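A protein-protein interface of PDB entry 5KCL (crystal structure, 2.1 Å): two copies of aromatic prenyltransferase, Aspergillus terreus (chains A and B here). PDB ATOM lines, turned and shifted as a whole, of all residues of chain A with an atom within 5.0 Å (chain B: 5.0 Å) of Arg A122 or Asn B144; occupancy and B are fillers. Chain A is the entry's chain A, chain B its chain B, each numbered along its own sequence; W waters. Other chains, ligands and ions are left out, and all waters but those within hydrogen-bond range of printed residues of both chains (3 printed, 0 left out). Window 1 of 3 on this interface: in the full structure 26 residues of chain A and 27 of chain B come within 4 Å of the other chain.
NE of Arg B122 is in salt-bridge range of OD1 of Asp B141 (2.7 Å). The guanidinium group of Arg A122 lies within salt-bridge range of the side-chain carboxylate of Asp A141 (2.7 Å).
Arg B122 touches its own counterpart, Arg A122. Asp A141 touches its own counterpart, Asp B141. Of the 7 pairs that touch across the chains among the printed residues, 2 have their exchanged pair printed and touching as well.
Printed residues of chain A that touch a printed residue of chain B: Arg A122, Arg A138 and Asp A141.
Arg A122 touches just these residues of chain B: Arg B122 (3.7 Å) and Asn B144 (3.4 Å). Asn B144 touches two residues of chain A. Of the printed residues of chain A, Arg B122 touches Arg A122 (3.7 Å). Printed residues of chain B within 4 Å of Asp A141: Asp B141, Asn B144 and Ala B145. The nearest printed residue of chain B that does not touch Arg A122 is Asp B141 (5.1 Å).
Water W1 lies within hydrogen-bond range of OD2 of Asp A141 (2.8 Å) and O of Asn B144 (3.0 Å). Water W2 bridges the backbone carbonyl oxygen (O) of Phe A119 (2.9 Å) and the guanidinium group (NH1) of Arg B122 (3.0 Å). Water W3 lies within hydrogen-bond range of the backbone carbonyl oxygen of Ser B118 (2.9 Å), the guanidinium group of Arg A122 (2.9 Å) and the side-chain amide oxygen of Asn B144 (3.0 Å).
Arg A122 touches Arg B122. Arg A138 touches Ala B145 (O to CB, 3.2 Å). Asp B141 touches Asp A141 (CB to O, 3.4 Å). CB of Asp A141 touches CB of Ala B145 (3.9 Å).
The guanidinium group of Arg A122 lies within hydrogen-bond range of the side-chain amide oxygen of Asn B144, 3.4 Å away. The side-chain carboxylate (OD2) of Asp A141 sits close to the side-chain amide oxygen (OD1) of Asn B144 (2.9 Å). NH1 of Arg A138 sits close to O of Gly B148.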
ATOM      1  N   PHE A 119     -17.789 -10.537  15.054  1.00  0.00           N
ATOM      2  CA  PHE A 119     -17.596 -11.992  15.161  1.00  0.00           C
ATOM      3  C   PHE A 119     -18.852 -12.852  14.915  1.00  0.00           C
ATOM      4  O   PHE A 119     -18.720 -14.025  14.518  1.00  0.00           O
ATOM      5  CB  PHE A 119     -17.042 -12.335  16.564  1.00  0.00           C
ATOM      6  CG  PHE A 119     -15.901 -11.439  17.026  1.00  0.00           C
ATOM      7  CD1 PHE A 119     -14.661 -11.498  16.411  1.00  0.00           C
ATOM      8  CD2 PHE A 119     -16.084 -10.544  18.072  1.00  0.00           C
ATOM      9  CE1 PHE A 119     -13.604 -10.643  16.755  1.00  0.00           C
ATOM     10  CE2 PHE A 119     -15.023  -9.714  18.471  1.00  0.00           C
ATOM     11  CZ  PHE A 119     -13.794  -9.753  17.807  1.00  0.00           C
ATOM     12  N   GLY A 120     -20.046 -12.306  15.181  1.00  0.00           N
ATOM     13  CA  GLY A 120     -21.270 -13.103  15.090  1.00  0.00           C
ATOM     14  C   GLY A 120     -21.445 -13.741  13.724  1.00  0.00           C
ATOM     15  O   GLY A 120     -21.821 -14.924  13.640  1.00  0.00           O
ATOM     16  N   ASP A 121     -21.191 -12.990  12.649  1.00  0.00           N
ATOM     17  CA  ASP A 121     -21.485 -13.509  11.287  1.00  0.00           C
ATOM     18  C   ASP A 121     -20.573 -14.756  10.954  1.00  0.00           C
ATOM     19  O   ASP A 121     -21.049 -15.735  10.498  1.00  0.00           O
ATOM     20  CB  ASP A 121     -21.469 -12.412  10.201  1.00  0.00           C
ATOM     21  CG  ASP A 121     -22.688 -11.407  10.317  1.00  0.00           C
ATOM     22  OD1 ASP A 121     -22.623 -10.464  11.146  1.00  0.00           O
ATOM     23  OD2 ASP A 121     -23.730 -11.516   9.555  1.00  0.00           O
ATOM     24  N   ARG A 122     -19.306 -14.704  11.318  1.00  0.00           N
ATOM     25  CA  ARG A 122     -18.390 -15.775  11.080  1.00  0.00           C
ATOM     26  C   ARG A 122     -18.755 -16.954  11.968  1.00  0.00           C
ATOM     27  O   ARG A 122     -18.688 -18.078  11.536  1.00  0.00           O
ATOM     28  CB  ARG A 122     -16.968 -15.294  11.341  1.00  0.00           C
ATOM     29  CG  ARG A 122     -15.809 -16.293  11.116  1.00  0.00           C
ATOM     30  CD  ARG A 122     -15.831 -16.901   9.741  1.00  0.00           C
ATOM     31  NE  ARG A 122     -14.617 -17.626   9.312  1.00  0.00           N
ATOM     32  CZ  ARG A 122     -14.228 -18.832   9.727  1.00  0.00           C
ATOM     33  NH1 ARG A 122     -14.878 -19.481  10.721  1.00  0.00           N
ATOM     34  NH2 ARG A 122     -13.186 -19.413   9.141  1.00  0.00           N
ATOM     35  N   GLU A 123     -19.166 -16.704  13.188  1.00  0.00           N
ATOM     36  CA  GLU A 123     -19.656 -17.814  14.000  1.00  0.00           C
ATOM     37  C   GLU A 123     -20.872 -18.519  13.338  1.00  0.00           C
ATOM     38  O   GLU A 123     -20.949 -19.753  13.334  1.00  0.00           O
ATOM     39  CB  GLU A 123     -20.003 -17.406  15.408  1.00  0.00           C
ATOM     40  CG  GLU A 123     -20.480 -18.653  16.167  1.00  0.00           C
ATOM     41  CD  GLU A 123     -20.858 -18.432  17.606  1.00  0.00           C
ATOM     42  OE1 GLU A 123     -20.409 -17.447  18.203  1.00  0.00           O
ATOM     43  OE2 GLU A 123     -21.614 -19.265  18.124  1.00  0.00           O
ATOM     44  N   LEU A 124     -21.850 -17.758  12.860  1.00  0.00           N
ATOM     45  CA  LEU A 124     -22.998 -18.370  12.143  1.00  0.00           C
ATOM     46  C   LEU A 124     -22.475 -19.155  10.936  1.00  0.00           C
ATOM     47  O   LEU A 124     -22.876 -20.242  10.678  1.00  0.00           O
ATOM     48  CB  LEU A 124     -23.991 -17.274  11.645  1.00  0.00           C
ATOM     49  CG  LEU A 124     -25.084 -17.764  10.693  1.00  0.00           C
ATOM     50  CD1 LEU A 124     -25.961 -18.808  11.340  1.00  0.00           C
ATOM     51  CD2 LEU A 124     -25.963 -16.584  10.318  1.00  0.00           C
ATOM     52  N   LEU A 125     -21.545 -18.585  10.198  1.00  0.00           N
ATOM     53  CA  LEU A 125     -21.076 -19.251   8.987  1.00  0.00           C
ATOM     54  C   LEU A 125     -20.298 -20.552   9.251  1.00  0.00           C
ATOM     55  O   LEU A 125     -20.421 -21.502   8.496  1.00  0.00           O
ATOM     56  CB  LEU A 125     -20.208 -18.316   8.173  1.00  0.00           C
ATOM     57  CG  LEU A 125     -21.103 -17.327   7.414  1.00  0.00           C
ATOM     58  CD1 LEU A 125     -20.386 -16.014   7.218  1.00  0.00           C
ATOM     59  CD2 LEU A 125     -21.489 -17.977   6.082  1.00  0.00           C
ATOM     60  N   LYS A 126     -19.581 -20.574  10.339  1.00  0.00           N
ATOM     61  CA  LYS A 126     -18.915 -21.779  10.801  1.00  0.00           C
ATOM     62  C   LYS A 126     -19.947 -22.884  11.040  1.00  0.00           C
ATOM     63  O   LYS A 126     -19.787 -23.970  10.559  1.00  0.00           O
ATOM     64  CB  LYS A 126     -18.094 -21.490  12.055  1.00  0.00           C
ATOM     65  CG  LYS A 126     -17.623 -22.751  12.762  1.00  0.00           C
ATOM     66  CD  LYS A 126     -17.521 -22.579  14.282  1.00  0.00           C
ATOM     67  CE  LYS A 126     -18.860 -22.779  14.927  1.00  0.00           C
ATOM     68  NZ  LYS A 126     -18.864 -22.323  16.336  1.00  0.00           N
ATOM     69  N   LEU A 137     -15.818 -20.788   3.181  1.00  0.00           N
ATOM     70  CA  LEU A 137     -15.574 -19.638   3.954  1.00  0.00           C
ATOM     71  C   LEU A 137     -14.407 -18.844   3.444  1.00  0.00           C
ATOM     72  O   LEU A 137     -14.035 -17.842   4.066  1.00  0.00           O
ATOM     73  CB  LEU A 137     -15.321 -20.026   5.407  1.00  0.00           C
ATOM     74  CG  LEU A 137     -16.478 -20.778   6.113  1.00  0.00           C
ATOM     75  CD1 LEU A 137     -16.160 -20.870   7.575  1.00  0.00           C
ATOM     76  CD2 LEU A 137     -17.843 -20.142   5.930  1.00  0.00           C
ATOM     77  N   ARG A 138     -13.811 -19.252   2.345  1.00  0.00           N
ATOM     78  CA  ARG A 138     -12.544 -18.620   1.916  1.00  0.00           C
ATOM     79  C   ARG A 138     -12.667 -17.197   1.515  1.00  0.00           C
ATOM     80  O   ARG A 138     -11.814 -16.402   1.869  1.00  0.00           O
ATOM     81  CB  ARG A 138     -11.824 -19.467   0.831  1.00  0.00           C
ATOM     82  CG  ARG A 138     -11.159 -20.699   1.485  1.00  0.00           C
ATOM     83  CD  ARG A 138     -10.626 -21.692   0.487  1.00  0.00           C
ATOM     84  NE  ARG A 138     -11.715 -22.270  -0.288  1.00  0.00           N
ATOM     85  CZ  ARG A 138     -11.602 -23.323  -1.103  1.00  0.00           C
ATOM     86  NH1 ARG A 138     -10.452 -23.954  -1.240  1.00  0.00           N
ATOM     87  NH2 ARG A 138     -12.657 -23.776  -1.751  1.00  0.00           N
ATOM     88  N   PHE A 140     -15.198 -15.223   2.507  1.00  0.00           N
ATOM     89  CA  PHE A 140     -15.493 -14.576   3.775  1.00  0.00           C
ATOM     90  C   PHE A 140     -14.189 -14.205   4.512  1.00  0.00           C
ATOM     91  O   PHE A 140     -14.001 -13.041   4.903  1.00  0.00           O
ATOM     92  CB  PHE A 140     -16.333 -15.446   4.660  1.00  0.00           C
ATOM     93  CG  PHE A 140     -16.729 -14.739   5.913  1.00  0.00           C
ATOM     94  CD1 PHE A 140     -15.814 -14.578   6.977  1.00  0.00           C
ATOM     95  CD2 PHE A 140     -17.941 -14.113   5.991  1.00  0.00           C
ATOM     96  CE1 PHE A 140     -16.133 -13.823   8.113  1.00  0.00           C
ATOM     97  CE2 PHE A 140     -18.286 -13.381   7.146  1.00  0.00           C
ATOM     98  CZ  PHE A 140     -17.393 -13.231   8.201  1.00  0.00           C
ATOM     99  N   ASP A 141     -13.303 -15.178   4.704  1.00  0.00           N
ATOM    100  CA  ASP A 141     -12.088 -14.931   5.442  1.00  0.00           C
ATOM    101  C   ASP A 141     -11.196 -13.914   4.730  1.00  0.00           C
ATOM    102  O   ASP A 141     -10.549 -13.030   5.336  1.00  0.00           O
ATOM    103  CB  ASP A 141     -11.345 -16.244   5.673  1.00  0.00           C
ATOM    104  CG  ASP A 141     -12.058 -17.150   6.694  1.00  0.00           C
ATOM    105  OD1 ASP A 141     -12.833 -16.649   7.529  1.00  0.00           O
ATOM    106  OD2 ASP A 141     -11.889 -18.405   6.658  1.00  0.00           O
ATOM    107  N   SER B 118     -11.254 -28.044  10.617  1.00  0.00           N
ATOM    108  CA  SER B 118     -11.024 -26.721  10.029  1.00  0.00           C
ATOM    109  C   SER B 118     -11.528 -25.534  10.818  1.00  0.00           C
ATOM    110  O   SER B 118     -11.301 -24.416  10.374  1.00  0.00           O
ATOM    111  CB  SER B 118     -11.694 -26.619   8.631  1.00  0.00           C
ATOM    112  OG  SER B 118     -11.056 -27.480   7.709  1.00  0.00           O
ATOM    113  N   ARG B 122     -10.246 -21.333  14.842  1.00  0.00           N
ATOM    114  CA  ARG B 122     -10.827 -19.988  14.620  1.00  0.00           C
ATOM    115  C   ARG B 122     -11.893 -19.721  15.704  1.00  0.00           C
ATOM    116  O   ARG B 122     -12.009 -18.607  16.184  1.00  0.00           O
ATOM    117  CB  ARG B 122     -11.395 -19.875  13.219  1.00  0.00           C
ATOM    118  CG  ARG B 122     -12.017 -18.530  12.779  1.00  0.00           C
ATOM    119  CD  ARG B 122     -11.109 -17.330  12.973  1.00  0.00           C
ATOM    120  NE  ARG B 122     -11.497 -16.047  12.324  1.00  0.00           N
ATOM    121  CZ  ARG B 122     -12.481 -15.211  12.726  1.00  0.00           C
ATOM    122  NH1 ARG B 122     -13.311 -15.545  13.740  1.00  0.00           N
ATOM    123  NH2 ARG B 122     -12.633 -14.030  12.113  1.00  0.00           N
ATOM    124  N   LEU B 139      -4.397 -11.648  10.123  1.00  0.00           N
ATOM    125  CA  LEU B 139      -3.483 -12.598   9.523  1.00  0.00           C
ATOM    126  C   LEU B 139      -3.975 -14.029   9.592  1.00  0.00           C
ATOM    127  O   LEU B 139      -3.819 -14.788   8.629  1.00  0.00           O
ATOM    128  CB  LEU B 139      -2.085 -12.461  10.108  1.00  0.00           C
ATOM    129  CG  LEU B 139      -1.351 -11.203   9.750  1.00  0.00           C
ATOM    130  CD1 LEU B 139      -0.022 -11.218  10.476  1.00  0.00           C
ATOM    131  CD2 LEU B 139      -1.092 -11.028   8.265  1.00  0.00           C
ATOM    132  N   PHE B 140      -4.618 -14.409  10.692  1.00  0.00           N
ATOM    133  CA  PHE B 140      -5.307 -15.647  10.713  1.00  0.00           C
ATOM    134  C   PHE B 140      -6.245 -15.789   9.495  1.00  0.00           C
ATOM    135  O   PHE B 140      -6.248 -16.815   8.790  1.00  0.00           O
ATOM    136  CB  PHE B 140      -6.118 -15.852  11.987  1.00  0.00           C
ATOM    137  CG  PHE B 140      -6.716 -17.237  12.049  1.00  0.00           C
ATOM    138  CD1 PHE B 140      -7.848 -17.561  11.335  1.00  0.00           C
ATOM    139  CD2 PHE B 140      -6.084 -18.229  12.746  1.00  0.00           C
ATOM    140  CE1 PHE B 140      -8.382 -18.843  11.336  1.00  0.00           C
ATOM    141  CE2 PHE B 140      -6.603 -19.524  12.760  1.00  0.00           C
ATOM    142  CZ  PHE B 140      -7.760 -19.843  12.061  1.00  0.00           C
ATOM    143  N   ASP B 141      -7.136 -14.826   9.321  1.00  0.00           N
ATOM    144  CA  ASP B 141      -8.174 -14.913   8.278  1.00  0.00           C
ATOM    145  C   ASP B 141      -7.509 -14.911   6.881  1.00  0.00           C
ATOM    146  O   ASP B 141      -7.933 -15.617   5.985  1.00  0.00           O
ATOM    147  CB  ASP B 141      -9.183 -13.738   8.422  1.00  0.00           C
ATOM    148  CG  ASP B 141     -10.122 -13.918   9.677  1.00  0.00           C
ATOM    149  OD1 ASP B 141     -10.293 -15.072  10.146  1.00  0.00           O
ATOM    150  OD2 ASP B 141     -10.612 -12.913  10.215  1.00  0.00           O
ATOM    151  N   HIS B 142      -6.450 -14.134   6.735  1.00  0.00           N
ATOM    152  CA  HIS B 142      -5.771 -14.097   5.458  1.00  0.00           C
ATOM    153  C   HIS B 142      -5.280 -15.481   5.081  1.00  0.00           C
ATOM    154  O   HIS B 142      -5.597 -15.981   4.016  1.00  0.00           O
ATOM    155  CB  HIS B 142      -4.601 -13.106   5.450  1.00  0.00           C
ATOM    156  CG  HIS B 142      -3.814 -13.182   4.193  1.00  0.00           C
ATOM    157  ND1 HIS B 142      -4.232 -12.575   3.028  1.00  0.00           N
ATOM    158  CD2 HIS B 142      -2.713 -13.909   3.880  1.00  0.00           C
ATOM    159  CE1 HIS B 142      -3.411 -12.903   2.057  1.00  0.00           C
ATOM    160  NE2 HIS B 142      -2.462 -13.683   2.552  1.00  0.00           N
ATOM    161  N   PHE B 143      -4.489 -16.103   5.943  1.00  0.00           N
ATOM    162  CA  PHE B 143      -3.956 -17.423   5.604  1.00  0.00           C
ATOM    163  C   PHE B 143      -4.980 -18.552   5.583  1.00  0.00           C
ATOM    164  O   PHE B 143      -4.854 -19.457   4.774  1.00  0.00           O
ATOM    165  CB  PHE B 143      -2.759 -17.747   6.488  1.00  0.00           C
ATOM    166  CG  PHE B 143      -1.557 -16.983   6.086  1.00  0.00           C
ATOM    167  CD1 PHE B 143      -0.901 -17.311   4.901  1.00  0.00           C
ATOM    168  CD2 PHE B 143      -1.142 -15.870   6.789  1.00  0.00           C
ATOM    169  CE1 PHE B 143       0.187 -16.561   4.481  1.00  0.00           C
ATOM    170  CE2 PHE B 143      -0.043 -15.122   6.381  1.00  0.00           C
ATOM    171  CZ  PHE B 143       0.614 -15.456   5.222  1.00  0.00           C
ATOM    172  N   ASN B 144      -6.031 -18.446   6.398  1.00  0.00           N
ATOM    173  CA  ASN B 144      -7.122 -19.370   6.305  1.00  0.00           C
ATOM    174  C   ASN B 144      -7.765 -19.312   4.925  1.00  0.00           C
ATOM    175  O   ASN B 144      -8.156 -20.334   4.403  1.00  0.00           O
ATOM    176  CB  ASN B 144      -8.205 -19.073   7.357  1.00  0.00           C
ATOM    177  CG  ASN B 144      -8.908 -20.302   7.800  1.00  0.00           C
ATOM    178  OD1 ASN B 144     -10.123 -20.298   7.931  1.00  0.00           O
ATOM    179  ND2 ASN B 144      -8.187 -21.387   7.942  1.00  0.00           N
ATOM    180  N   ALA B 145      -7.914 -18.112   4.373  1.00  0.00           N
ATOM    181  CA  ALA B 145      -8.494 -17.976   3.042  1.00  0.00           C
ATOM    182  C   ALA B 145      -7.557 -18.565   1.979  1.00  0.00           C
ATOM    183  O   ALA B 145      -8.028 -19.166   1.052  1.00  0.00           O
ATOM    184  CB  ALA B 145      -8.762 -16.530   2.700  1.00  0.00           C
ATOM    185  N   GLN B 146      -6.242 -18.424   2.161  1.00  0.00           N
ATOM    186  CA  GLN B 146      -5.276 -18.877   1.164  1.00  0.00           C
ATOM    187  C   GLN B 146      -5.015 -20.385   1.182  1.00  0.00           C
ATOM    188  O   GLN B 146      -4.807 -20.935   0.131  1.00  0.00           O
ATOM    189  CB  GLN B 146      -3.937 -18.113   1.275  1.00  0.00           C
ATOM    190  CG  GLN B 146      -4.036 -16.590   1.230  1.00  0.00           C
ATOM    191  CD  GLN B 146      -4.739 -16.028   0.019  1.00  0.00           C
ATOM    192  OE1 GLN B 146      -5.706 -15.232   0.119  1.00  0.00           O
ATOM    193  NE2 GLN B 146      -4.217 -16.366  -1.124  1.00  0.00           N
ATOM    194  N   VAL B 147      -4.970 -21.034   2.356  1.00  0.00           N
ATOM    195  CA  VAL B 147      -4.558 -22.444   2.451  1.00  0.00           C
ATOM    196  C   VAL B 147      -5.657 -23.374   2.990  1.00  0.00           C
ATOM    197  O   VAL B 147      -5.473 -24.556   3.019  1.00  0.00           O
ATOM    198  CB  VAL B 147      -3.182 -22.665   3.114  1.00  0.00           C
ATOM    199  CG1 VAL B 147      -2.117 -21.779   2.452  1.00  0.00           C
ATOM    200  CG2 VAL B 147      -3.199 -22.426   4.593  1.00  0.00           C
ATOM    201  N   GLY B 148      -6.839 -22.824   3.269  1.00  0.00           N
ATOM    202  CA  GLY B 148      -8.002 -23.607   3.722  1.00  0.00           C
ATOM    203  C   GLY B 148      -8.689 -24.287   2.577  1.00  0.00           C
ATOM    204  O   GLY B 148      -8.464 -23.956   1.421  1.00  0.00           O
ATOM    205  N   PHE B 186      -0.185 -22.598   9.774  1.00  0.00           N
ATOM    206  CA  PHE B 186      -1.032 -23.192   8.731  1.00  0.00           C
ATOM    207  C   PHE B 186      -0.202 -24.170   7.917  1.00  0.00           C
ATOM    208  O   PHE B 186       0.892 -23.819   7.479  1.00  0.00           O
ATOM    209  CB  PHE B 186      -1.521 -22.097   7.824  1.00  0.00           C
ATOM    210  CG  PHE B 186      -2.504 -21.185   8.477  1.00  0.00           C
ATOM    211  CD1 PHE B 186      -2.085 -20.087   9.208  1.00  0.00           C
ATOM    212  CD2 PHE B 186      -3.857 -21.464   8.398  1.00  0.00           C
ATOM    213  CE1 PHE B 186      -3.029 -19.241   9.784  1.00  0.00           C
ATOM    214  CE2 PHE B 186      -4.788 -20.641   8.997  1.00  0.00           C
ATOM    215  CZ  PHE B 186      -4.381 -19.525   9.680  1.00  0.00           C
HETATM  216  O   HOH W   1     -11.181 -20.121   4.599  1.00  0.00           O
HETATM  217  O   HOH W   2     -16.144 -15.272  14.516  1.00  0.00           O
HETATM  218  O   HOH W   3     -12.287 -22.180   8.811  1.00  0.00           O
